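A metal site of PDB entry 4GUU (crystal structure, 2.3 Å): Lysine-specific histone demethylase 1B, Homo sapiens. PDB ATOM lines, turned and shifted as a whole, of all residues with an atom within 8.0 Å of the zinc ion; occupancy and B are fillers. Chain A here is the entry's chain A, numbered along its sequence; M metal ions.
O of Lys 103 lies within hydrogen-bond range of N of Cys 96 (2.9 Å).
The guanidinium group of Arg 102 lies within hydrogen-bond range of the backbone carbonyl oxygen of Cys 96, at 3.0 Å.
The backbone carbonyl oxygen (O) of Cys 139 is in hydrogen-bond range of the side-chain amino group (NZ) of Lys 103.
The side-chain sulfur of Cys 101 lies close to the backbone NH of Lys 103, 3.6 Å away.
The guanidinium group of Arg 105 sits close to the side-chain sulfur of Cys 123.
The side-chain sulfur (SG) of Cys 96 lies close to the backbone NH (N) of Lys 98 (3.5 Å).
The zinc ion is bound by the side-chain sulfur (SG) of Cys 101, 2.4 Å away.
The side-chain sulfur (SG) of Cys 96 is bound to the zinc ion (2.5 Å).
The zinc ion is bound by the side-chain sulfur (SG) of Cys 123, 2.5 Å away.
The zinc ion is bound by the side-chain sulfur (SG) of Cys 139 (2.5 Å).
The zinc ion has four donor atoms within binding distance.
Of the 20 residues printed, 4 come within 4 Å of the zinc ion.
The nearest printed residue that does not touch the zinc ion is Lys 98 (4.6 Å).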
ATOM      1  N   GLN A  95     -16.241 -22.054 -11.430  1.00  0.00           N
ATOM      2  CA  GLN A  95     -16.003 -23.435 -11.033  1.00  0.00           C
ATOM      3  C   GLN A  95     -16.382 -24.413 -12.138  1.00  0.00           C
ATOM      4  O   GLN A  95     -17.431 -24.284 -12.756  1.00  0.00           O
ATOM      5  CB  GLN A  95     -16.764 -23.761  -9.762  1.00  0.00           C
ATOM      6  CG  GLN A  95     -16.338 -25.060  -9.098  1.00  0.00           C
ATOM      7  CD  GLN A  95     -16.952 -25.224  -7.718  1.00  0.00           C
ATOM      8  OE1 GLN A  95     -17.863 -24.483  -7.347  1.00  0.00           O
ATOM      9  NE2 GLN A  95     -16.450 -26.187  -6.956  1.00  0.00           N
ATOM     10  N   CYS A  96     -15.504 -25.383 -12.384  1.00  0.00           N
ATOM     11  CA  CYS A  96     -15.761 -26.404 -13.394  1.00  0.00           C
ATOM     12  C   CYS A  96     -16.945 -27.267 -12.985  1.00  0.00           C
ATOM     13  O   CYS A  96     -17.069 -27.670 -11.821  1.00  0.00           O
ATOM     14  CB  CYS A  96     -14.508 -27.274 -13.590  1.00  0.00           C
ATOM     15  SG  CYS A  96     -14.716 -28.655 -14.742  1.00  0.00           S
ATOM     16  N   THR A  97     -17.822 -27.548 -13.934  1.00  0.00           N
ATOM     17  CA  THR A  97     -19.067 -28.257 -13.661  1.00  0.00           C
ATOM     18  C   THR A  97     -18.968 -29.776 -13.837  1.00  0.00           C
ATOM     19  O   THR A  97     -19.949 -30.496 -13.630  1.00  0.00           O
ATOM     20  CB  THR A  97     -20.227 -27.731 -14.521  1.00  0.00           C
ATOM     21  OG1 THR A  97     -19.908 -27.866 -15.914  1.00  0.00           O
ATOM     22  CG2 THR A  97     -20.491 -26.262 -14.206  1.00  0.00           C
ATOM     23  N   LYS A  98     -17.787 -30.248 -14.237  1.00  0.00           N
ATOM     24  CA  LYS A  98     -17.543 -31.676 -14.313  1.00  0.00           C
ATOM     25  C   LYS A  98     -17.559 -32.216 -12.883  1.00  0.00           C
ATOM     26  O   LYS A  98     -16.776 -31.775 -12.046  1.00  0.00           O
ATOM     27  CB  LYS A  98     -16.192 -31.955 -14.967  1.00  0.00           C
ATOM     28  CG  LYS A  98     -15.936 -33.432 -15.222  1.00  0.00           C
ATOM     29  CD  LYS A  98     -14.612 -33.652 -15.937  1.00  0.00           C
ATOM     30  CE  LYS A  98     -14.318 -35.129 -16.084  1.00  0.00           C
ATOM     31  NZ  LYS A  98     -12.984 -35.378 -16.692  1.00  0.00           N
ATOM     32  N   PRO A  99     -18.452 -33.173 -12.614  1.00  0.00           N
ATOM     33  CA  PRO A  99     -18.693 -33.664 -11.248  1.00  0.00           C
ATOM     34  C   PRO A  99     -17.436 -34.212 -10.562  1.00  0.00           C
ATOM     35  O   PRO A  99     -17.309 -34.072  -9.340  1.00  0.00           O
ATOM     36  CB  PRO A  99     -19.723 -34.780 -11.452  1.00  0.00           C
ATOM     37  CG  PRO A  99     -20.385 -34.451 -12.747  1.00  0.00           C
ATOM     38  CD  PRO A  99     -19.307 -33.850 -13.596  1.00  0.00           C
ATOM     39  N   GLU A 100     -16.537 -34.825 -11.320  1.00  0.00           N
ATOM     40  CA  GLU A 100     -15.332 -35.415 -10.745  1.00  0.00           C
ATOM     41  C   GLU A 100     -14.194 -34.410 -10.586  1.00  0.00           C
ATOM     42  O   GLU A 100     -13.181 -34.703  -9.956  1.00  0.00           O
ATOM     43  CB  GLU A 100     -14.856 -36.609 -11.571  1.00  0.00           C
ATOM     44  CG  GLU A 100     -15.168 -36.506 -13.048  1.00  0.00           C
ATOM     45  CD  GLU A 100     -16.449 -37.226 -13.411  1.00  0.00           C
ATOM     46  OE1 GLU A 100     -16.982 -36.994 -14.527  1.00  0.00           O
ATOM     47  OE2 GLU A 100     -16.928 -38.041 -12.593  1.00  0.00           O
ATOM     48  N   CYS A 101     -14.351 -33.220 -11.166  1.00  0.00           N
ATOM     49  CA  CYS A 101     -13.313 -32.194 -11.096  1.00  0.00           C
ATOM     50  C   CYS A 101     -13.673 -31.127 -10.075  1.00  0.00           C
ATOM     51  O   CYS A 101     -13.098 -31.071  -8.986  1.00  0.00           O
ATOM     52  CB  CYS A 101     -13.056 -31.561 -12.465  1.00  0.00           C
ATOM     53  SG  CYS A 101     -11.801 -30.255 -12.449  1.00  0.00           S
ATOM     54  N   ARG A 102     -14.621 -30.265 -10.424  1.00  0.00           N
ATOM     55  CA  ARG A 102     -15.126 -29.244  -9.518  1.00  0.00           C
ATOM     56  C   ARG A 102     -14.075 -28.246  -9.067  1.00  0.00           C
ATOM     57  O   ARG A 102     -14.232 -27.591  -8.037  1.00  0.00           O
ATOM     58  CB  ARG A 102     -15.787 -29.901  -8.298  1.00  0.00           C
ATOM     59  CG  ARG A 102     -16.990 -30.745  -8.643  1.00  0.00           C
ATOM     60  CD  ARG A 102     -18.078 -29.885  -9.284  1.00  0.00           C
ATOM     61  NE  ARG A 102     -18.693 -28.983  -8.322  1.00  0.00           N
ATOM     62  CZ  ARG A 102     -19.266 -27.820  -8.636  1.00  0.00           C
ATOM     63  NH1 ARG A 102     -19.798 -27.060  -7.690  1.00  0.00           N
ATOM     64  NH2 ARG A 102     -19.292 -27.415  -9.897  1.00  0.00           N
ATOM     65  N   LYS A 103     -13.009 -28.111  -9.844  1.00  0.00           N
ATOM     66  CA  LYS A 103     -11.948 -27.162  -9.513  1.00  0.00           C
ATOM     67  C   LYS A 103     -12.297 -25.750  -9.966  1.00  0.00           C
ATOM     68  O   LYS A 103     -12.957 -25.562 -10.996  1.00  0.00           O
ATOM     69  CB  LYS A 103     -10.608 -27.604 -10.116  1.00  0.00           C
ATOM     70  CG  LYS A 103     -10.059 -28.884  -9.502  1.00  0.00           C
ATOM     71  CD  LYS A 103      -8.550 -28.997  -9.693  1.00  0.00           C
ATOM     72  CE  LYS A 103      -8.192 -29.708 -10.992  1.00  0.00           C
ATOM     73  NZ  LYS A 103      -8.562 -31.154 -10.944  1.00  0.00           N
ATOM     74  N   TRP A 104     -11.863 -24.760  -9.189  1.00  0.00           N
ATOM     75  CA  TRP A 104     -12.081 -23.358  -9.524  1.00  0.00           C
ATOM     76  C   TRP A 104     -10.990 -22.840 -10.456  1.00  0.00           C
ATOM     77  O   TRP A 104      -9.818 -23.179 -10.271  1.00  0.00           O
ATOM     78  CB  TRP A 104     -12.099 -22.509  -8.247  1.00  0.00           C
ATOM     79  CG  TRP A 104     -13.404 -22.511  -7.523  1.00  0.00           C
ATOM     80  CD1 TRP A 104     -13.780 -23.353  -6.515  1.00  0.00           C
ATOM     81  CD2 TRP A 104     -14.502 -21.612  -7.743  1.00  0.00           C
ATOM     82  NE1 TRP A 104     -15.053 -23.031  -6.095  1.00  0.00           N
ATOM     83  CE2 TRP A 104     -15.509 -21.973  -6.828  1.00  0.00           C
ATOM     84  CE3 TRP A 104     -14.722 -20.548  -8.617  1.00  0.00           C
ATOM     85  CZ2 TRP A 104     -16.733 -21.300  -6.772  1.00  0.00           C
ATOM     86  CZ3 TRP A 104     -15.925 -19.883  -8.554  1.00  0.00           C
ATOM     87  CH2 TRP A 104     -16.917 -20.259  -7.633  1.00  0.00           C
ATOM     88  N   ARG A 105     -11.364 -22.029 -11.440  1.00  0.00           N
ATOM     89  CA  ARG A 105     -10.390 -21.532 -12.415  1.00  0.00           C
ATOM     90  C   ARG A 105     -10.525 -20.032 -12.634  1.00  0.00           C
ATOM     91  O   ARG A 105     -11.624 -19.485 -12.666  1.00  0.00           O
ATOM     92  CB  ARG A 105     -10.561 -22.241 -13.757  1.00  0.00           C
ATOM     93  CG  ARG A 105     -10.892 -23.714 -13.666  1.00  0.00           C
ATOM     94  CD  ARG A 105      -9.778 -24.585 -14.223  1.00  0.00           C
ATOM     95  NE  ARG A 105      -8.652 -24.733 -13.301  1.00  0.00           N
ATOM     96  CZ  ARG A 105      -7.855 -25.801 -13.268  1.00  0.00           C
ATOM     97  NH1 ARG A 105      -8.067 -26.817 -14.100  1.00  0.00           N
ATOM     98  NH2 ARG A 105      -6.854 -25.861 -12.404  1.00  0.00           N
ATOM     99  N   TYR A 121     -19.769 -24.253 -17.533  1.00  0.00           N
ATOM    100  CA  TYR A 121     -18.319 -24.167 -17.602  1.00  0.00           C
ATOM    101  C   TYR A 121     -17.589 -25.440 -17.185  1.00  0.00           C
ATOM    102  O   TYR A 121     -17.937 -26.080 -16.194  1.00  0.00           O
ATOM    103  CB  TYR A 121     -17.787 -22.992 -16.778  1.00  0.00           C
ATOM    104  CG  TYR A 121     -16.281 -22.923 -16.773  1.00  0.00           C
ATOM    105  CD1 TYR A 121     -15.536 -23.556 -15.789  1.00  0.00           C
ATOM    106  CD2 TYR A 121     -15.591 -22.232 -17.768  1.00  0.00           C
ATOM    107  CE1 TYR A 121     -14.150 -23.506 -15.785  1.00  0.00           C
ATOM    108  CE2 TYR A 121     -14.207 -22.167 -17.773  1.00  0.00           C
ATOM    109  CZ  TYR A 121     -13.490 -22.815 -16.778  1.00  0.00           C
ATOM    110  OH  TYR A 121     -12.117 -22.766 -16.763  1.00  0.00           O
ATOM    111  N   ARG A 122     -16.562 -25.782 -17.959  1.00  0.00           N
ATOM    112  CA  ARG A 122     -15.564 -26.757 -17.518  1.00  0.00           C
ATOM    113  C   ARG A 122     -14.161 -26.348 -17.976  1.00  0.00           C
ATOM    114  O   ARG A 122     -14.000 -25.686 -18.998  1.00  0.00           O
ATOM    115  CB  ARG A 122     -15.899 -28.192 -17.947  1.00  0.00           C
ATOM    116  CG  ARG A 122     -16.772 -28.325 -19.172  1.00  0.00           C
ATOM    117  CD  ARG A 122     -17.653 -29.576 -19.062  1.00  0.00           C
ATOM    118  NE  ARG A 122     -16.872 -30.803 -18.958  1.00  0.00           N
ATOM    119  CZ  ARG A 122     -17.356 -31.972 -18.550  1.00  0.00           C
ATOM    120  NH1 ARG A 122     -18.637 -32.072 -18.184  1.00  0.00           N
ATOM    121  NH2 ARG A 122     -16.579 -33.036 -18.494  1.00  0.00           N
ATOM    122  N   CYS A 123     -13.156 -26.725 -17.194  1.00  0.00           N
ATOM    123  CA  CYS A 123     -11.769 -26.323 -17.438  1.00  0.00           C
ATOM    124  C   CYS A 123     -11.405 -26.256 -18.910  1.00  0.00           C
ATOM    125  O   CYS A 123     -11.696 -27.164 -19.680  1.00  0.00           O
ATOM    126  CB  CYS A 123     -10.810 -27.281 -16.728  1.00  0.00           C
ATOM    127  SG  CYS A 123     -10.988 -27.322 -14.935  1.00  0.00           S
ATOM    128  N   GLY A 124     -10.757 -25.156 -19.302  1.00  0.00           N
ATOM    129  CA  GLY A 124     -10.254 -25.007 -20.654  1.00  0.00           C
ATOM    130  C   GLY A 124     -11.159 -24.267 -21.620  1.00  0.00           C
ATOM    131  O   GLY A 124     -10.719 -23.820 -22.675  1.00  0.00           O
ATOM    132  N   ASP A 137      -6.492 -31.998 -21.890  1.00  0.00           N
ATOM    133  CA  ASP A 137      -6.588 -32.580 -20.560  1.00  0.00           C
ATOM    134  C   ASP A 137      -6.584 -31.457 -19.523  1.00  0.00           C
ATOM    135  O   ASP A 137      -5.861 -31.522 -18.524  1.00  0.00           O
ATOM    136  CB  ASP A 137      -5.414 -33.530 -20.282  1.00  0.00           C
ATOM    137  CG  ASP A 137      -5.864 -34.894 -19.801  1.00  0.00           C
ATOM    138  OD1 ASP A 137      -6.853 -34.966 -19.033  1.00  0.00           O
ATOM    139  OD2 ASP A 137      -5.241 -35.897 -20.200  1.00  0.00           O
ATOM    140  N   HIS A 138      -7.399 -30.434 -19.762  1.00  0.00           N
ATOM    141  CA  HIS A 138      -7.399 -29.227 -18.938  1.00  0.00           C
ATOM    142  C   HIS A 138      -7.757 -29.444 -17.466  1.00  0.00           C
ATOM    143  O   HIS A 138      -7.260 -28.738 -16.599  1.00  0.00           O
ATOM    144  CB  HIS A 138      -8.327 -28.174 -19.558  1.00  0.00           C
ATOM    145  CG  HIS A 138      -7.932 -27.755 -20.946  1.00  0.00           C
ATOM    146  ND1 HIS A 138      -6.804 -26.984 -21.180  1.00  0.00           N
ATOM    147  CD2 HIS A 138      -8.497 -27.990 -22.141  1.00  0.00           C
ATOM    148  CE1 HIS A 138      -6.701 -26.769 -22.488  1.00  0.00           C
ATOM    149  NE2 HIS A 138      -7.705 -27.363 -23.092  1.00  0.00           N
ATOM    150  N   CYS A 139      -8.607 -30.432 -17.193  1.00  0.00           N
ATOM    151  CA  CYS A 139      -9.103 -30.659 -15.842  1.00  0.00           C
ATOM    152  C   CYS A 139      -8.035 -31.208 -14.896  1.00  0.00           C
ATOM    153  O   CYS A 139      -8.179 -31.133 -13.678  1.00  0.00           O
ATOM    154  CB  CYS A 139     -10.313 -31.610 -15.856  1.00  0.00           C
ATOM    155  SG  CYS A 139     -11.845 -30.894 -16.527  1.00  0.00           S
ATOM    156  N   SER A 140      -6.969 -31.756 -15.458  1.00  0.00           N
ATOM    157  CA  SER A 140      -5.927 -32.388 -14.641  1.00  0.00           C
ATOM    158  C   SER A 140      -4.978 -31.378 -13.988  1.00  0.00           C
ATOM    159  O   SER A 140      -4.435 -31.633 -12.916  1.00  0.00           O
ATOM    160  CB  SER A 140      -5.144 -33.411 -15.462  1.00  0.00           C
ATOM    161  OG  SER A 140      -4.599 -32.809 -16.628  1.00  0.00           O
ATOM    162  N   LEU A 141      -4.780 -30.235 -14.647  1.00  0.00           N
ATOM    163  CA  LEU A 141      -3.928 -29.179 -14.121  1.00  0.00           C
ATOM    164  C   LEU A 141      -4.321 -28.811 -12.702  1.00  0.00           C
ATOM    165  O   LEU A 141      -5.505 -28.721 -12.381  1.00  0.00           O
ATOM    166  CB  LEU A 141      -3.986 -27.949 -15.029  1.00  0.00           C
ATOM    167  CG  LEU A 141      -3.647 -28.217 -16.502  1.00  0.00           C
ATOM    168  CD1 LEU A 141      -3.849 -26.970 -17.355  1.00  0.00           C
ATOM    169  CD2 LEU A 141      -2.231 -28.754 -16.649  1.00  0.00           C
HETATM  170 ZN    ZN M   1     -12.371 -29.387 -14.573  1.00  0.00          ZN
